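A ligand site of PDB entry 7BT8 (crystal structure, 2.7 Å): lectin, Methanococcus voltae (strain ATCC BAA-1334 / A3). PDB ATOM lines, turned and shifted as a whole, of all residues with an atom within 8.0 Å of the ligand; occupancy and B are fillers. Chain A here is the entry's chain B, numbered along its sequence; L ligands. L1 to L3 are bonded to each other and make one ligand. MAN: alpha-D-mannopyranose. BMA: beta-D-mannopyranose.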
ATOM      1  N   GLY A  11      20.671   9.852  15.100  1.00  0.00           N
ATOM      2  CA  GLY A  11      19.299   9.519  15.526  1.00  0.00           C
ATOM      3  C   GLY A  11      18.305  10.608  15.186  1.00  0.00           C
ATOM      4  O   GLY A  11      18.723  11.620  14.627  1.00  0.00           O
ATOM      5  N   VAL A  12      17.036  10.396  15.569  1.00  0.00           N
ATOM      6  CA  VAL A  12      15.871  11.260  15.225  1.00  0.00           C
ATOM      7  C   VAL A  12      15.569  12.230  16.380  1.00  0.00           C
ATOM      8  O   VAL A  12      14.771  13.149  16.173  1.00  0.00           O
ATOM      9  CB  VAL A  12      14.651  10.379  14.907  1.00  0.00           C
ATOM     10  CG1 VAL A  12      14.860   9.604  13.605  1.00  0.00           C
ATOM     11  CG2 VAL A  12      14.331   9.450  16.065  1.00  0.00           C
ATOM     12  N   GLY A  13      16.197  12.021  17.550  1.00  0.00           N
ATOM     13  CA  GLY A  13      16.031  12.845  18.762  1.00  0.00           C
ATOM     14  C   GLY A  13      16.490  14.276  18.582  1.00  0.00           C
ATOM     15  O   GLY A  13      17.016  14.610  17.513  1.00  0.00           O
ATOM     16  N   GLY A  14      16.271  15.104  19.600  1.00  0.00           N
ATOM     17  CA  GLY A  14      16.726  16.508  19.695  1.00  0.00           C
ATOM     18  C   GLY A  14      15.902  17.487  18.861  1.00  0.00           C
ATOM     19  O   GLY A  14      15.131  17.084  17.949  1.00  0.00           O
ATOM     20  N   THR A  15      16.087  18.768  19.143  1.00  0.00           N
ATOM     21  CA  THR A  15      15.415  19.876  18.412  1.00  0.00           C
ATOM     22  C   THR A  15      16.119  20.087  17.071  1.00  0.00           C
ATOM     23  O   THR A  15      17.303  20.373  17.029  1.00  0.00           O
ATOM     24  CB  THR A  15      15.462  21.169  19.231  1.00  0.00           C
ATOM     25  OG1 THR A  15      15.024  20.891  20.565  1.00  0.00           O
ATOM     26  CG2 THR A  15      14.620  22.273  18.612  1.00  0.00           C
ATOM     27  N   PRO A  16      15.406  20.020  15.935  1.00  0.00           N
ATOM     28  CA  PRO A  16      15.980  20.399  14.654  1.00  0.00           C
ATOM     29  C   PRO A  16      16.738  21.729  14.753  1.00  0.00           C
ATOM     30  O   PRO A  16      16.297  22.546  15.487  1.00  0.00           O
ATOM     31  CB  PRO A  16      14.766  20.594  13.728  1.00  0.00           C
ATOM     32  CG  PRO A  16      13.703  19.697  14.330  1.00  0.00           C
ATOM     33  CD  PRO A  16      13.982  19.646  15.822  1.00  0.00           C
ATOM     34  N   LEU A  39      30.602  11.125  22.557  1.00  0.00           N
ATOM     35  CA  LEU A  39      29.703  11.771  21.558  1.00  0.00           C
ATOM     36  C   LEU A  39      30.093  13.240  21.397  1.00  0.00           C
ATOM     37  O   LEU A  39      30.758  13.819  22.301  1.00  0.00           O
ATOM     38  CB  LEU A  39      28.254  11.798  22.039  1.00  0.00           C
ATOM     39  CG  LEU A  39      27.701  10.576  22.755  1.00  0.00           C
ATOM     40  CD1 LEU A  39      26.251  10.795  23.123  1.00  0.00           C
ATOM     41  CD2 LEU A  39      27.817   9.348  21.881  1.00  0.00           C
ATOM     42  N   LEU A  40      29.542  13.853  20.353  1.00  0.00           N
ATOM     43  CA  LEU A  40      29.504  15.332  20.213  1.00  0.00           C
ATOM     44  C   LEU A  40      28.362  15.809  21.093  1.00  0.00           C
ATOM     45  O   LEU A  40      27.330  15.115  21.088  1.00  0.00           O
ATOM     46  CB  LEU A  40      29.265  15.720  18.753  1.00  0.00           C
ATOM     47  CG  LEU A  40      30.400  15.399  17.771  1.00  0.00           C
ATOM     48  CD1 LEU A  40      30.341  16.349  16.583  1.00  0.00           C
ATOM     49  CD2 LEU A  40      31.771  15.501  18.404  1.00  0.00           C
ATOM     50  N   HIS A  41      28.545  16.910  21.820  1.00  0.00           N
ATOM     51  CA  HIS A  41      27.494  17.511  22.683  1.00  0.00           C
ATOM     52  C   HIS A  41      27.003  18.875  22.151  1.00  0.00           C
ATOM     53  O   HIS A  41      25.840  19.203  22.389  1.00  0.00           O
ATOM     54  CB  HIS A  41      28.011  17.610  24.103  1.00  0.00           C
ATOM     55  CG  HIS A  41      28.284  16.283  24.729  1.00  0.00           C
ATOM     56  ND1 HIS A  41      27.291  15.358  24.945  1.00  0.00           N
ATOM     57  CD2 HIS A  41      29.421  15.755  25.240  1.00  0.00           C
ATOM     58  CE1 HIS A  41      27.811  14.304  25.556  1.00  0.00           C
ATOM     59  NE2 HIS A  41      29.134  14.525  25.732  1.00  0.00           N
ATOM     60  N   GLY A  57      22.931  22.223  20.975  1.00  0.00           N
ATOM     61  CA  GLY A  57      23.401  21.225  21.945  1.00  0.00           C
ATOM     62  C   GLY A  57      23.875  21.864  23.230  1.00  0.00           C
ATOM     63  O   GLY A  57      23.879  23.106  23.330  1.00  0.00           O
ATOM     64  N   ASP A  58      24.296  21.038  24.178  1.00  0.00           N
ATOM     65  CA  ASP A  58      24.688  21.438  25.555  1.00  0.00           C
ATOM     66  C   ASP A  58      26.207  21.342  25.643  1.00  0.00           C
ATOM     67  O   ASP A  58      26.763  20.266  25.408  1.00  0.00           O
ATOM     68  CB  ASP A  58      23.920  20.530  26.514  1.00  0.00           C
ATOM     69  CG  ASP A  58      24.230  20.771  27.978  1.00  0.00           C
ATOM     70  OD1 ASP A  58      25.176  21.528  28.255  1.00  0.00           O
ATOM     71  OD2 ASP A  58      23.517  20.192  28.821  1.00  0.00           O
ATOM     72  N   LYS A  60      28.663  20.459  27.390  1.00  0.00           N
ATOM     73  CA  LYS A  60      28.946  19.753  28.665  1.00  0.00           C
ATOM     74  C   LYS A  60      30.265  18.988  28.565  1.00  0.00           C
ATOM     75  O   LYS A  60      30.805  18.641  29.615  1.00  0.00           O
ATOM     76  CB  LYS A  60      27.766  18.858  29.075  1.00  0.00           C
ATOM     77  CG  LYS A  60      27.444  17.703  28.139  1.00  0.00           C
ATOM     78  CD  LYS A  60      26.042  17.115  28.354  1.00  0.00           C
ATOM     79  CE  LYS A  60      25.971  16.111  29.485  1.00  0.00           C
ATOM     80  NZ  LYS A  60      24.739  15.305  29.416  1.00  0.00           N
ATOM     81  N   ASN A  86      17.409   4.974  15.251  1.00  0.00           N
ATOM     82  CA  ASN A  86      16.514   6.039  15.776  1.00  0.00           C
ATOM     83  C   ASN A  86      17.158   6.627  17.026  1.00  0.00           C
ATOM     84  O   ASN A  86      17.170   7.854  17.108  1.00  0.00           O
ATOM     85  CB  ASN A  86      15.106   5.526  16.086  1.00  0.00           C
ATOM     86  CG  ASN A  86      14.374   5.071  14.840  1.00  0.00           C
ATOM     87  OD1 ASN A  86      14.442   5.711  13.791  1.00  0.00           O
ATOM     88  ND2 ASN A  86      13.652   3.963  14.960  1.00  0.00           N
ATOM     89  N   ASP A  87      17.715   5.810  17.915  1.00  0.00           N
ATOM     90  CA  ASP A  87      18.364   6.291  19.168  1.00  0.00           C
ATOM     91  C   ASP A  87      19.839   6.655  18.884  1.00  0.00           C
ATOM     92  O   ASP A  87      20.669   6.630  19.828  1.00  0.00           O
ATOM     93  CB  ASP A  87      18.185   5.282  20.298  1.00  0.00           C
ATOM     94  CG  ASP A  87      18.349   5.901  21.676  1.00  0.00           C
ATOM     95  OD1 ASP A  87      18.169   7.141  21.804  1.00  0.00           O
ATOM     96  OD2 ASP A  87      18.663   5.148  22.621  1.00  0.00           O
ATOM     97  N   GLY A  88      20.129   7.008  17.622  1.00  0.00           N
ATOM     98  CA  GLY A  88      21.467   7.346  17.119  1.00  0.00           C
ATOM     99  C   GLY A  88      21.987   8.672  17.650  1.00  0.00           C
ATOM    100  O   GLY A  88      21.179   9.496  18.130  1.00  0.00           O
ATOM    101  N   ARG A  89      23.309   8.854  17.582  1.00  0.00           N
ATOM    102  CA  ARG A  89      24.054  10.069  17.979  1.00  0.00           C
ATOM    103  C   ARG A  89      25.173  10.308  16.973  1.00  0.00           C
ATOM    104  O   ARG A  89      25.621   9.363  16.329  1.00  0.00           O
ATOM    105  CB  ARG A  89      24.671   9.902  19.363  1.00  0.00           C
ATOM    106  CG  ARG A  89      23.652   9.756  20.471  1.00  0.00           C
ATOM    107  CD  ARG A  89      22.911  11.040  20.782  1.00  0.00           C
ATOM    108  NE  ARG A  89      22.175  10.839  22.014  1.00  0.00           N
ATOM    109  CZ  ARG A  89      21.038  10.169  22.107  1.00  0.00           C
ATOM    110  NH1 ARG A  89      20.441   9.675  21.035  1.00  0.00           N
ATOM    111  NH2 ARG A  89      20.491  10.009  23.291  1.00  0.00           N
ATOM    112  N   GLY A 126      19.783  17.685  14.471  1.00  0.00           N
ATOM    113  CA  GLY A 126      19.018  17.786  15.725  1.00  0.00           C
ATOM    114  C   GLY A 126      19.956  17.630  16.890  1.00  0.00           C
ATOM    115  O   GLY A 126      20.955  16.842  16.754  1.00  0.00           O
ATOM    116  N   ALA A 127      19.691  18.366  17.971  1.00  0.00           N
ATOM    117  CA  ALA A 127      20.486  18.307  19.215  1.00  0.00           C
ATOM    118  C   ALA A 127      19.574  18.644  20.395  1.00  0.00           C
ATOM    119  O   ALA A 127      18.663  19.460  20.184  1.00  0.00           O
ATOM    120  CB  ALA A 127      21.656  19.269  19.149  1.00  0.00           C
ATOM    121  N   GLY A 128      19.833  17.997  21.534  1.00  0.00           N
ATOM    122  CA  GLY A 128      19.505  18.497  22.877  1.00  0.00           C
ATOM    123  C   GLY A 128      20.704  18.477  23.818  1.00  0.00           C
ATOM    124  O   GLY A 128      21.537  19.418  23.764  1.00  0.00           O
ATOM    125  N   SER A 129      20.783  17.461  24.682  1.00  0.00           N
ATOM    126  CA  SER A 129      21.966  17.226  25.545  1.00  0.00           C
ATOM    127  C   SER A 129      23.172  16.919  24.662  1.00  0.00           C
ATOM    128  O   SER A 129      24.307  17.233  25.045  1.00  0.00           O
ATOM    129  CB  SER A 129      21.710  16.094  26.503  1.00  0.00           C
ATOM    130  OG  SER A 129      20.977  16.558  27.627  1.00  0.00           O
ATOM    131  N   ASP A 130      22.902  16.253  23.540  1.00  0.00           N
ATOM    132  CA  ASP A 130      23.906  15.672  22.629  1.00  0.00           C
ATOM    133  C   ASP A 130      23.611  16.220  21.231  1.00  0.00           C
ATOM    134  O   ASP A 130      22.520  16.829  21.025  1.00  0.00           O
ATOM    135  CB  ASP A 130      23.853  14.140  22.682  1.00  0.00           C
ATOM    136  CG  ASP A 130      23.942  13.524  24.077  1.00  0.00           C
ATOM    137  OD1 ASP A 130      24.608  14.120  24.954  1.00  0.00           O
ATOM    138  OD2 ASP A 130      23.363  12.417  24.275  1.00  0.00           O
ATOM    139  N   ILE A 131      24.555  16.039  20.301  1.00  0.00           N
ATOM    140  CA  ILE A 131      24.285  16.191  18.845  1.00  0.00           C
ATOM    141  C   ILE A 131      23.686  14.857  18.404  1.00  0.00           C
ATOM    142  O   ILE A 131      24.410  13.829  18.423  1.00  0.00           O
ATOM    143  CB  ILE A 131      25.546  16.546  18.048  1.00  0.00           C
ATOM    144  CG1 ILE A 131      26.274  17.737  18.690  1.00  0.00           C
ATOM    145  CG2 ILE A 131      25.188  16.772  16.575  1.00  0.00           C
ATOM    146  CD1 ILE A 131      25.514  19.063  18.684  1.00  0.00           C
ATOM    147  N   ASP A 132      22.401  14.889  18.108  1.00  0.00           N
ATOM    148  CA  ASP A 132      21.613  13.702  17.743  1.00  0.00           C
ATOM    149  C   ASP A 132      22.007  13.336  16.317  1.00  0.00           C
ATOM    150  O   ASP A 132      22.442  12.190  16.070  1.00  0.00           O
ATOM    151  CB  ASP A 132      20.108  13.923  17.939  1.00  0.00           C
ATOM    152  CG  ASP A 132      19.718  13.979  19.410  1.00  0.00           C
ATOM    153  OD1 ASP A 132      19.873  15.078  20.001  1.00  0.00           O
ATOM    154  OD2 ASP A 132      19.309  12.911  19.957  1.00  0.00           O
ATOM    155  N   ARG A 133      21.916  14.314  15.430  1.00  0.00           N
ATOM    156  CA  ARG A 133      22.182  14.089  13.998  1.00  0.00           C
ATOM    157  C   ARG A 133      22.885  15.307  13.411  1.00  0.00           C
ATOM    158  O   ARG A 133      22.639  16.410  13.895  1.00  0.00           O
ATOM    159  CB  ARG A 133      20.848  13.836  13.332  1.00  0.00           C
ATOM    160  CG  ARG A 133      20.923  13.403  11.884  1.00  0.00           C
ATOM    161  CD  ARG A 133      19.482  13.463  11.360  1.00  0.00           C
ATOM    162  NE  ARG A 133      18.746  14.756  11.423  1.00  0.00           N
ATOM    163  CZ  ARG A 133      17.587  15.048  12.072  1.00  0.00           C
ATOM    164  NH1 ARG A 133      16.899  14.169  12.774  1.00  0.00           N
ATOM    165  NH2 ARG A 133      17.027  16.232  11.924  1.00  0.00           N
HETATM  166  C1  MAN L   1      17.042  15.998  24.772  1.00  0.00           C
HETATM  167  C2  MAN L   1      16.107  15.949  23.582  1.00  0.00           C
HETATM  168  C3  MAN L   1      16.110  14.523  22.975  1.00  0.00           C
HETATM  169  C4  MAN L   1      17.535  14.090  22.672  1.00  0.00           C
HETATM  170  C5  MAN L   1      18.374  14.211  23.943  1.00  0.00           C
HETATM  171  C6  MAN L   1      19.840  13.858  23.662  1.00  0.00           C
HETATM  172  O2  MAN L   1      16.579  16.977  22.679  1.00  0.00           O
HETATM  173  O3  MAN L   1      15.371  14.542  21.768  1.00  0.00           O
HETATM  174  O4  MAN L   1      17.603  12.777  22.202  1.00  0.00           O
HETATM  175  O5  MAN L   1      18.359  15.587  24.403  1.00  0.00           O
HETATM  176  O6  MAN L   1      20.376  14.674  22.599  1.00  0.00           O
HETATM  177  C1  BMA L   2      17.976  14.299  29.174  1.00  0.00           C
HETATM  178  C2  BMA L   2      17.835  14.067  27.643  1.00  0.00           C
HETATM  179  C3  BMA L   2      17.259  15.331  27.048  1.00  0.00           C
HETATM  180  C4  BMA L   2      16.066  15.874  27.865  1.00  0.00           C
HETATM  181  C5  BMA L   2      16.305  15.926  29.263  1.00  0.00           C
HETATM  182  C6  BMA L   2      14.964  16.363  29.843  1.00  0.00           C
HETATM  183  O1  BMA L   2      18.524  13.155  29.864  1.00  0.00           O
HETATM  184  O2  BMA L   2      16.988  12.874  27.408  1.00  0.00           O
HETATM  185  O3  BMA L   2      16.772  14.992  25.737  1.00  0.00           O
HETATM  186  O4  BMA L   2      15.736  17.238  27.528  1.00  0.00           O
HETATM  187  O5  BMA L   2      16.654  14.599  29.720  1.00  0.00           O
HETATM  188  O6  BMA L   2      14.305  15.203  30.355  1.00  0.00           O
HETATM  189  C1  MAN L   3      14.717  14.687  31.652  1.00  0.00           C
HETATM  190  C2  MAN L   3      13.841  13.549  32.013  1.00  0.00           C
HETATM  191  C3  MAN L   3      12.394  14.033  32.088  1.00  0.00           C
HETATM  192  C4  MAN L   3      12.230  15.241  32.998  1.00  0.00           C
HETATM  193  C5  MAN L   3      13.340  16.271  32.763  1.00  0.00           C
HETATM  194  C6  MAN L   3      13.549  17.233  33.935  1.00  0.00           C
HETATM  195  O2  MAN L   3      14.271  12.977  33.263  1.00  0.00           O
HETATM  196  O3  MAN L   3      11.550  12.985  32.574  1.00  0.00           O
HETATM  197  O4  MAN L   3      10.940  15.844  32.767  1.00  0.00           O
HETATM  198  O5  MAN L   3      14.592  15.610  32.729  1.00  0.00           O
HETATM  199  O6  MAN L   3      12.272  17.742  34.299  1.00  0.00           O
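N of Gly 11 is in hydrogen-bond range of O of Asp 132 (3.1 Å). The backbone NH (N) of Thr 15 lies within hydrogen-bond range of the backbone carbonyl oxygen (O) of Ala 127 (2.9 Å). The guanidinium group of Arg 89 is in salt-bridge range of the side-chain carboxylate of Asp 130, at 3.0 Å. O of Gly 128 sits at hydrogen-bond distance from N of Asp 58, at 3.2 Å. The side-chain carboxylate (OD1) of Asp 130 is in hydrogen-bond range of a ring nitrogen (ND1) of His 41 (3.0 Å). The backbone NH of Gly 128 lies within hydrogen-bond range of the side-chain carboxylate of Asp 132 (3.3 Å). NH1 of Arg 89 lies within salt-bridge range of OD1 of Asp 87 (3.5 Å). The backbone NH (N) of Asp 132 is in hydrogen-bond range of the backbone carbonyl oxygen (O) of Gly 126 (2.8 Å).
O6 of MAN L1 lies within hydrogen-bond range of OD1 of Asp 132 (2.7 Å). An oxygen (O6) of MAN L1 sits at hydrogen-bond distance from the backbone NH of Asp 130, at 3.1 Å. O6 of MAN L1 lies within hydrogen-bond range of O of Asp 130 (3.4 Å). The backbone NH (N) of Ser 129 sits at hydrogen-bond distance from an oxygen (O5) of MAN L1, at 3.1 Å. An oxygen (O3) of MAN L1 sits at hydrogen-bond distance from the backbone NH (N) of Gly 14, 2.4 Å away.
C of Gly 13 touches O3 of MAN L1, at 3.4 Å. N of Thr 15 touches O2 of MAN L1, 3.99 Å away. NH2 of Arg 89 touches C6 of MAN L1, at 3.9 Å. CA of Gly 128 touches O2 of MAN L1, at 3.3 Å. Within 4 Å of the ligand: Gly 13, Gly 14, Thr 15, Arg 89, Gly 128, Ser 129, Asp 130 and Asp 132. The nearest printed residue that does not touch the ligand is Ala 127 (4.1 Å).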
